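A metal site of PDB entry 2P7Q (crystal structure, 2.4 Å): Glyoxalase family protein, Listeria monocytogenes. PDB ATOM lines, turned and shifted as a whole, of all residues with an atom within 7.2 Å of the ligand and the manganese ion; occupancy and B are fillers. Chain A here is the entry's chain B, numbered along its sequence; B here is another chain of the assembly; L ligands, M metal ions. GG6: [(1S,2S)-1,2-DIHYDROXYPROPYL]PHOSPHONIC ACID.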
ATOM      1  N   TYR A  67      18.142  21.587  -3.299  1.00  0.00           N
ATOM      2  CA  TYR A  67      18.209  20.998  -1.965  1.00  0.00           C
ATOM      3  C   TYR A  67      17.042  21.327  -1.046  1.00  0.00           C
ATOM      4  O   TYR A  67      17.073  21.017   0.134  1.00  0.00           O
ATOM      5  CB  TYR A  67      19.524  21.366  -1.290  1.00  0.00           C
ATOM      6  CG  TYR A  67      19.881  20.441  -0.145  1.00  0.00           C
ATOM      7  CD1 TYR A  67      20.159  19.086  -0.374  1.00  0.00           C
ATOM      8  CD2 TYR A  67      19.979  20.911   1.164  1.00  0.00           C
ATOM      9  CE1 TYR A  67      20.523  18.232   0.670  1.00  0.00           C
ATOM     10  CE2 TYR A  67      20.343  20.070   2.218  1.00  0.00           C
ATOM     11  CZ  TYR A  67      20.621  18.730   1.963  1.00  0.00           C
ATOM     12  OH  TYR A  67      21.008  17.899   2.996  1.00  0.00           O
ATOM     13  N   HIS A  69      13.656  20.749   0.630  1.00  0.00           N
ATOM     14  CA  HIS A  69      13.027  19.469   0.890  1.00  0.00           C
ATOM     15  C   HIS A  69      12.012  19.451   2.016  1.00  0.00           C
ATOM     16  O   HIS A  69      11.896  20.409   2.798  1.00  0.00           O
ATOM     17  CB  HIS A  69      14.094  18.395   1.152  1.00  0.00           C
ATOM     18  CG  HIS A  69      15.043  18.713   2.261  1.00  0.00           C
ATOM     19  ND1 HIS A  69      16.205  19.432   2.060  1.00  0.00           N
ATOM     20  CD2 HIS A  69      15.039  18.378   3.579  1.00  0.00           C
ATOM     21  CE1 HIS A  69      16.882  19.513   3.195  1.00  0.00           C
ATOM     22  NE2 HIS A  69      16.185  18.881   4.131  1.00  0.00           N
ATOM     23  N   ILE A  70      11.267  18.340   2.077  1.00  0.00           N
ATOM     24  CA  ILE A  70      10.264  18.108   3.097  1.00  0.00           C
ATOM     25  C   ILE A  70      10.763  16.879   3.831  1.00  0.00           C
ATOM     26  O   ILE A  70      11.152  15.898   3.199  1.00  0.00           O
ATOM     27  CB  ILE A  70       8.909  17.828   2.471  1.00  0.00           C
ATOM     28  CG1 ILE A  70       8.509  18.990   1.555  1.00  0.00           C
ATOM     29  CG2 ILE A  70       7.861  17.635   3.554  1.00  0.00           C
ATOM     30  CD1 ILE A  70       7.230  18.781   0.816  1.00  0.00           C
ATOM     31  N   ALA A  71      10.775  16.927   5.159  1.00  0.00           N
ATOM     32  CA  ALA A  71      11.267  15.789   5.928  1.00  0.00           C
ATOM     33  C   ALA A  71      10.224  15.262   6.888  1.00  0.00           C
ATOM     34  O   ALA A  71       9.493  16.038   7.518  1.00  0.00           O
ATOM     35  CB  ALA A  71      12.513  16.186   6.687  1.00  0.00           C
ATOM     36  N   GLY A 104      20.450  12.323  15.034  1.00  0.00           N
ATOM     37  CA  GLY A 104      20.033  11.086  14.404  1.00  0.00           C
ATOM     38  C   GLY A 104      20.306  10.971  12.917  1.00  0.00           C
ATOM     39  O   GLY A 104      20.739  11.925  12.265  1.00  0.00           O
ATOM     40  N   ARG A 105      20.039   9.777  12.379  1.00  0.00           N
ATOM     41  CA  ARG A 105      20.246   9.480  10.975  1.00  0.00           C
ATOM     42  C   ARG A 105      19.096   9.966  10.096  1.00  0.00           C
ATOM     43  O   ARG A 105      17.987  10.221  10.581  1.00  0.00           O
ATOM     44  CB  ARG A 105      20.421   7.974  10.812  1.00  0.00           C
ATOM     45  CG  ARG A 105      21.437   7.352  11.757  1.00  0.00           C
ATOM     46  CD  ARG A 105      21.197   5.858  11.936  1.00  0.00           C
ATOM     47  NE  ARG A 105      21.503   5.077  10.741  1.00  0.00           N
ATOM     48  CZ  ARG A 105      21.296   3.758  10.629  1.00  0.00           C
ATOM     49  NH1 ARG A 105      20.784   3.081  11.653  1.00  0.00           N
ATOM     50  NH2 ARG A 105      21.616   3.137   9.513  1.00  0.00           N
ATOM     51  N   SER A 106      19.370  10.100   8.807  1.00  0.00           N
ATOM     52  CA  SER A 106      18.357  10.553   7.857  1.00  0.00           C
ATOM     53  C   SER A 106      18.508   9.870   6.503  1.00  0.00           C
ATOM     54  O   SER A 106      19.538   9.250   6.220  1.00  0.00           O
ATOM     55  CB  SER A 106      18.460  12.082   7.674  1.00  0.00           C
ATOM     56  OG  SER A 106      17.982  12.773   8.816  1.00  0.00           O
ATOM     57  N   TYR A 108      17.810  10.788   2.391  1.00  0.00           N
ATOM     58  CA  TYR A 108      17.394  11.720   1.364  1.00  0.00           C
ATOM     59  C   TYR A 108      17.136  10.951   0.082  1.00  0.00           C
ATOM     60  O   TYR A 108      17.883  10.049  -0.264  1.00  0.00           O
ATOM     61  CB  TYR A 108      18.475  12.778   1.118  1.00  0.00           C
ATOM     62  CG  TYR A 108      18.618  13.796   2.229  1.00  0.00           C
ATOM     63  CD1 TYR A 108      19.141  13.443   3.472  1.00  0.00           C
ATOM     64  CD2 TYR A 108      18.222  15.109   2.043  1.00  0.00           C
ATOM     65  CE1 TYR A 108      19.260  14.373   4.500  1.00  0.00           C
ATOM     66  CE2 TYR A 108      18.329  16.055   3.061  1.00  0.00           C
ATOM     67  CZ  TYR A 108      18.857  15.687   4.285  1.00  0.00           C
ATOM     68  OH  TYR A 108      18.964  16.620   5.292  1.00  0.00           O
ATOM     69  N   GLU A 118      13.037  13.444   2.659  1.00  0.00           N
ATOM     70  CA  GLU A 118      13.918  12.954   3.691  1.00  0.00           C
ATOM     71  C   GLU A 118      13.105  12.324   4.816  1.00  0.00           C
ATOM     72  O   GLU A 118      11.990  12.750   5.106  1.00  0.00           O
ATOM     73  CB  GLU A 118      14.763  14.085   4.270  1.00  0.00           C
ATOM     74  CG  GLU A 118      15.784  13.619   5.289  1.00  0.00           C
ATOM     75  CD  GLU A 118      16.274  14.744   6.169  1.00  0.00           C
ATOM     76  OE1 GLU A 118      16.353  15.887   5.675  1.00  0.00           O
ATOM     77  OE2 GLU A 118      16.582  14.492   7.357  1.00  0.00           O
ATOM     78  N   LEU A 119      13.673  11.273   5.408  1.00  0.00           N
ATOM     79  CA  LEU A 119      13.055  10.598   6.529  1.00  0.00           C
ATOM     80  C   LEU A 119      14.103  10.844   7.606  1.00  0.00           C
ATOM     81  O   LEU A 119      15.267  10.501   7.441  1.00  0.00           O
ATOM     82  CB  LEU A 119      12.896   9.093   6.261  1.00  0.00           C
ATOM     83  CG  LEU A 119      12.004   8.693   5.077  1.00  0.00           C
ATOM     84  CD1 LEU A 119      11.710   7.211   5.180  1.00  0.00           C
ATOM     85  CD2 LEU A 119      10.703   9.494   5.084  1.00  0.00           C
ATOM     86  N   HIS A 120      13.685  11.462   8.700  1.00  0.00           N
ATOM     87  CA  HIS A 120      14.631  11.806   9.742  1.00  0.00           C
ATOM     88  C   HIS A 120      14.388  11.181  11.104  1.00  0.00           C
ATOM     89  O   HIS A 120      13.292  11.258  11.667  1.00  0.00           O
ATOM     90  CB  HIS A 120      14.680  13.340   9.878  1.00  0.00           C
ATOM     91  CG  HIS A 120      15.543  13.814  11.008  1.00  0.00           C
ATOM     92  ND1 HIS A 120      16.907  13.601  11.036  1.00  0.00           N
ATOM     93  CD2 HIS A 120      15.237  14.437  12.158  1.00  0.00           C
ATOM     94  CE1 HIS A 120      17.396  14.082  12.155  1.00  0.00           C
ATOM     95  NE2 HIS A 120      16.407  14.594  12.862  1.00  0.00           N
ATOM     96  N   ARG A 127      18.250  17.444  18.374  1.00  0.00           N
ATOM     97  CA  ARG A 127      19.089  18.253  17.485  1.00  0.00           C
ATOM     98  C   ARG A 127      19.746  19.457  18.169  1.00  0.00           C
ATOM     99  O   ARG A 127      20.949  19.695  17.984  1.00  0.00           O
ATOM    100  CB  ARG A 127      18.251  18.722  16.288  1.00  0.00           C
ATOM    101  CG  ARG A 127      19.026  19.497  15.233  1.00  0.00           C
ATOM    102  CD  ARG A 127      20.331  18.803  14.848  1.00  0.00           C
ATOM    103  NE  ARG A 127      20.701  19.049  13.468  1.00  0.00           N
ATOM    104  CZ  ARG A 127      20.131  18.436  12.428  1.00  0.00           C
ATOM    105  NH1 ARG A 127      19.175  17.547  12.622  1.00  0.00           N
ATOM    106  NH2 ARG A 127      20.522  18.733  11.194  1.00  0.00           N
ATOM    107  N   SER B   6       8.779  16.253  10.062  1.00  0.00           N
ATOM    108  CA  SER B   6      10.013  16.502  10.789  1.00  0.00           C
ATOM    109  C   SER B   6      10.346  17.973  10.692  1.00  0.00           C
ATOM    110  O   SER B   6      10.404  18.683  11.687  1.00  0.00           O
ATOM    111  CB  SER B   6      11.159  15.698  10.214  1.00  0.00           C
ATOM    112  OG  SER B   6      12.350  15.951  10.948  1.00  0.00           O
ATOM    113  N   HIS B   7      10.545  18.419   9.453  1.00  0.00           N
ATOM    114  CA  HIS B   7      10.892  19.806   9.176  1.00  0.00           C
ATOM    115  C   HIS B   7      10.857  20.067   7.677  1.00  0.00           C
ATOM    116  O   HIS B   7      10.705  19.136   6.884  1.00  0.00           O
ATOM    117  CB  HIS B   7      12.298  20.116   9.712  1.00  0.00           C
ATOM    118  CG  HIS B   7      13.377  19.279   9.105  1.00  0.00           C
ATOM    119  ND1 HIS B   7      13.761  18.059   9.631  1.00  0.00           N
ATOM    120  CD2 HIS B   7      14.160  19.481   8.015  1.00  0.00           C
ATOM    121  CE1 HIS B   7      14.741  17.558   8.893  1.00  0.00           C
ATOM    122  NE2 HIS B   7      15.003  18.395   7.907  1.00  0.00           N
ATOM    123  N   ILE B   8      11.001  21.326   7.304  1.00  0.00           N
ATOM    124  CA  ILE B   8      11.006  21.735   5.905  1.00  0.00           C
ATOM    125  C   ILE B   8      12.200  22.666   5.729  1.00  0.00           C
ATOM    126  O   ILE B   8      12.331  23.663   6.425  1.00  0.00           O
ATOM    127  CB  ILE B   8       9.701  22.489   5.554  1.00  0.00           C
ATOM    128  CG1 ILE B   8       8.500  21.566   5.810  1.00  0.00           C
ATOM    129  CG2 ILE B   8       9.742  22.948   4.113  1.00  0.00           C
ATOM    130  CD1 ILE B   8       7.155  22.167   5.471  1.00  0.00           C
ATOM    131  N   THR B   9      13.076  22.318   4.801  1.00  0.00           N
ATOM    132  CA  THR B   9      14.267  23.110   4.575  1.00  0.00           C
ATOM    133  C   THR B   9      14.215  23.864   3.259  1.00  0.00           C
ATOM    134  O   THR B   9      14.127  23.258   2.195  1.00  0.00           O
ATOM    135  CB  THR B   9      15.536  22.228   4.566  1.00  0.00           C
ATOM    136  OG1 THR B   9      15.718  21.628   5.849  1.00  0.00           O
ATOM    137  CG2 THR B   9      16.769  23.035   4.196  1.00  0.00           C
ATOM    138  N   LEU B  10      14.275  25.184   3.327  1.00  0.00           N
ATOM    139  CA  LEU B  10      14.263  25.993   2.109  1.00  0.00           C
ATOM    140  C   LEU B  10      15.671  26.530   1.869  1.00  0.00           C
ATOM    141  O   LEU B  10      16.453  26.708   2.797  1.00  0.00           O
ATOM    142  CB  LEU B  10      13.283  27.140   2.237  1.00  0.00           C
ATOM    143  CG  LEU B  10      11.846  26.702   2.483  1.00  0.00           C
ATOM    144  CD1 LEU B  10      10.941  27.929   2.532  1.00  0.00           C
ATOM    145  CD2 LEU B  10      11.405  25.730   1.375  1.00  0.00           C
ATOM    146  N   SER B  42      27.441  25.306   6.917  1.00  0.00           N
ATOM    147  CA  SER B  42      26.852  26.350   6.100  1.00  0.00           C
ATOM    148  C   SER B  42      26.091  27.348   6.933  1.00  0.00           C
ATOM    149  O   SER B  42      25.750  27.104   8.085  1.00  0.00           O
ATOM    150  CB  SER B  42      25.949  25.748   5.041  1.00  0.00           C
ATOM    151  OG  SER B  42      24.998  24.905   5.668  1.00  0.00           O
ATOM    152  N   GLU B  44      23.061  29.028   8.200  1.00  0.00           N
ATOM    153  CA  GLU B  44      21.657  28.653   8.290  1.00  0.00           C
ATOM    154  C   GLU B  44      20.963  29.006   9.597  1.00  0.00           C
ATOM    155  O   GLU B  44      21.601  29.252  10.625  1.00  0.00           O
ATOM    156  CB  GLU B  44      21.525  27.151   8.054  1.00  0.00           C
ATOM    157  CG  GLU B  44      22.346  26.319   9.028  1.00  0.00           C
ATOM    158  CD  GLU B  44      22.059  24.832   8.938  1.00  0.00           C
ATOM    159  OE1 GLU B  44      22.164  24.254   7.836  1.00  0.00           O
ATOM    160  OE2 GLU B  44      21.704  24.243   9.980  1.00  0.00           O
ATOM    161  N   PHE B  46      17.162  28.140  12.018  1.00  0.00           N
ATOM    162  CA  PHE B  46      15.997  27.307  12.266  1.00  0.00           C
ATOM    163  C   PHE B  46      14.928  28.135  12.956  1.00  0.00           C
ATOM    164  O   PHE B  46      15.221  28.885  13.882  1.00  0.00           O
ATOM    165  CB  PHE B  46      16.350  26.139  13.198  1.00  0.00           C
ATOM    166  CG  PHE B  46      17.419  25.224  12.665  1.00  0.00           C
ATOM    167  CD1 PHE B  46      17.992  24.269  13.512  1.00  0.00           C
ATOM    168  CD2 PHE B  46      17.847  25.308  11.345  1.00  0.00           C
ATOM    169  CE1 PHE B  46      18.970  23.401  13.032  1.00  0.00           C
ATOM    170  CE2 PHE B  46      18.830  24.440  10.857  1.00  0.00           C
ATOM    171  CZ  PHE B  46      19.404  23.484  11.703  1.00  0.00           C
ATOM    172  N   TRP B  53       8.810  23.156  12.265  1.00  0.00           N
ATOM    173  CA  TRP B  53      10.234  23.418  12.337  1.00  0.00           C
ATOM    174  C   TRP B  53      10.740  23.776  10.920  1.00  0.00           C
ATOM    175  O   TRP B  53      10.917  22.909  10.073  1.00  0.00           O
ATOM    176  CB  TRP B  53      10.934  22.174  12.895  1.00  0.00           C
ATOM    177  CG  TRP B  53      12.436  22.161  12.854  1.00  0.00           C
ATOM    178  CD1 TRP B  53      13.263  23.225  12.623  1.00  0.00           C
ATOM    179  CD2 TRP B  53      13.294  21.027  13.045  1.00  0.00           C
ATOM    180  NE1 TRP B  53      14.582  22.825  12.650  1.00  0.00           N
ATOM    181  CE2 TRP B  53      14.636  21.474  12.915  1.00  0.00           C
ATOM    182  CE3 TRP B  53      13.073  19.663  13.311  1.00  0.00           C
ATOM    183  CZ2 TRP B  53      15.735  20.620  13.029  1.00  0.00           C
ATOM    184  CZ3 TRP B  53      14.174  18.813  13.439  1.00  0.00           C
ATOM    185  CH2 TRP B  53      15.484  19.303  13.294  1.00  0.00           C
ATOM    186  N   CYS B  55      13.615  25.323   8.354  1.00  0.00           N
ATOM    187  CA  CYS B  55      15.038  25.549   8.243  1.00  0.00           C
ATOM    188  C   CYS B  55      15.371  26.345   6.991  1.00  0.00           C
ATOM    189  O   CYS B  55      14.848  26.087   5.911  1.00  0.00           O
ATOM    190  CB  CYS B  55      15.798  24.231   8.197  1.00  0.00           C
ATOM    191  SG  CYS B  55      15.719  23.313   9.720  1.00  0.00           S
ATOM    192  N   ILE B  56      16.255  27.337   7.142  1.00  0.00           N
ATOM    193  CA  ILE B  56      16.678  28.179   6.048  1.00  0.00           C
ATOM    194  C   ILE B  56      18.194  28.066   5.891  1.00  0.00           C
ATOM    195  O   ILE B  56      18.938  28.245   6.855  1.00  0.00           O
ATOM    196  CB  ILE B  56      16.279  29.655   6.314  1.00  0.00           C
ATOM    197  CG1 ILE B  56      14.771  29.754   6.577  1.00  0.00           C
ATOM    198  CG2 ILE B  56      16.629  30.509   5.116  1.00  0.00           C
ATOM    199  CD1 ILE B  56      13.886  29.344   5.388  1.00  0.00           C
ATOM    200  N   MET B  57      18.641  27.742   4.688  1.00  0.00           N
ATOM    201  CA  MET B  57      20.060  27.593   4.378  1.00  0.00           C
ATOM    202  C   MET B  57      20.408  28.510   3.223  1.00  0.00           C
ATOM    203  O   MET B  57      19.603  28.700   2.314  1.00  0.00           O
ATOM    204  CB  MET B  57      20.385  26.171   3.968  1.00  0.00           C
ATOM    205  CG  MET B  57      20.452  25.186   5.108  1.00  0.00           C
ATOM    206  SD  MET B  57      21.004  23.579   4.485  1.00  0.00           S
ATOM    207  CE  MET B  57      22.703  23.912   4.116  1.00  0.00           C
HETATM  208  O1  GG6 L   1      17.803  17.215   7.486  1.00  0.00           O
HETATM  209  C2  GG6 L   1      18.864  17.550   8.402  1.00  0.00           C
HETATM  210  C3  GG6 L   1      19.814  16.313   8.572  1.00  0.00           C
HETATM  211  C1  GG6 L   1      19.705  18.775   7.879  1.00  0.00           C
HETATM  212  O2  GG6 L   1      20.386  18.541   6.638  1.00  0.00           O
HETATM  213  P   GG6 L   1      18.729  20.254   7.691  1.00  0.00           P
HETATM  214  O3  GG6 L   1      17.939  20.524   9.036  1.00  0.00           O
HETATM  215  O4  GG6 L   1      19.637  21.340   7.442  1.00  0.00           O
HETATM  216  O5  GG6 L   1      17.717  20.141   6.490  1.00  0.00           O
HETATM  217 MN    MN M   1      16.655  18.132   6.316  1.00  0.00          MN
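OH of Tyr 108 sits at hydrogen-bond distance from O2 of the ligand, 2.7 Å away. An oxygen (O5) of the ligand lies close to the side-chain hydroxyl (OG1) of Thr 9 of chain B (2.6 Å). O3 of the ligand is in salt-bridge range of NH2 of Arg 127 (3.8 Å). The side-chain sulfur of Cys 55 of chain B is in hydrogen-bond range of an oxygen (O3) of the ligand (3.6 Å).
O of His 7 of chain B is in hydrogen-bond range of N of Ala 71. ND1 of His 7 of chain B lies within hydrogen-bond range of OG of Ser 6 of chain B. The side-chain carboxylate of Glu 118 lies close to the side-chain hydroxyl of Tyr 108. The side-chain carboxylate (OE2) of Glu 118 lies within hydrogen-bond range of the side-chain hydroxyl (OG) of Ser 106 (2.7 Å). O of Thr 9 of chain B lies within hydrogen-bond range of N of His 69. The backbone NH (N) of Cys 55 of chain B is in hydrogen-bond range of the backbone carbonyl oxygen (O) of Ile 8 of chain B (2.9 Å). O of Cys 55 of chain B is in hydrogen-bond range of N of Leu 10 of chain B (2.8 Å). A ring nitrogen (ND1) of His 120 is in hydrogen-bond range of the side-chain hydroxyl of Ser 106 (2.6 Å).
Merely in contact with the ligand: Tyr 67 (3.8 Å), Glu 44 of chain B (3.9 Å), Met 57 of chain B (3.95 Å) and Ser 106 (3.99 Å). Hydrophobic or aromatic side chains that line the ligand: His 69, Tyr 108, His 7 of chain B and Met 57 of chain B. Along chain A the residues within 4 Å of the ligand span positions 67 to 127. The nearest printed residue that does not touch the ligand is Phe 46 of chain B (4.2 Å).
OG1 of Thr 9 of chain B touches the manganese ion (3.6 Å). Five residues have an atom within 4 Å of the manganese ion: His 69, Tyr 108, Glu 118, His 7 of chain B and Thr 9 of chain B.
The manganese ion is bound by an oxygen (O1) of the ligand (1.9 Å), an oxygen (O5) of the ligand (2.3 Å), a ring nitrogen (NE2) of His 7 of chain B (2.3 Å), the side-chain carboxylate of Glu 118 (2.4 Å) and a ring nitrogen (NE2) of His 69 (2.4 Å). The manganese ion has five donor atoms within binding distance. Slightly farther from the manganese ion lies OH of Tyr 108 (2.9 Å).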
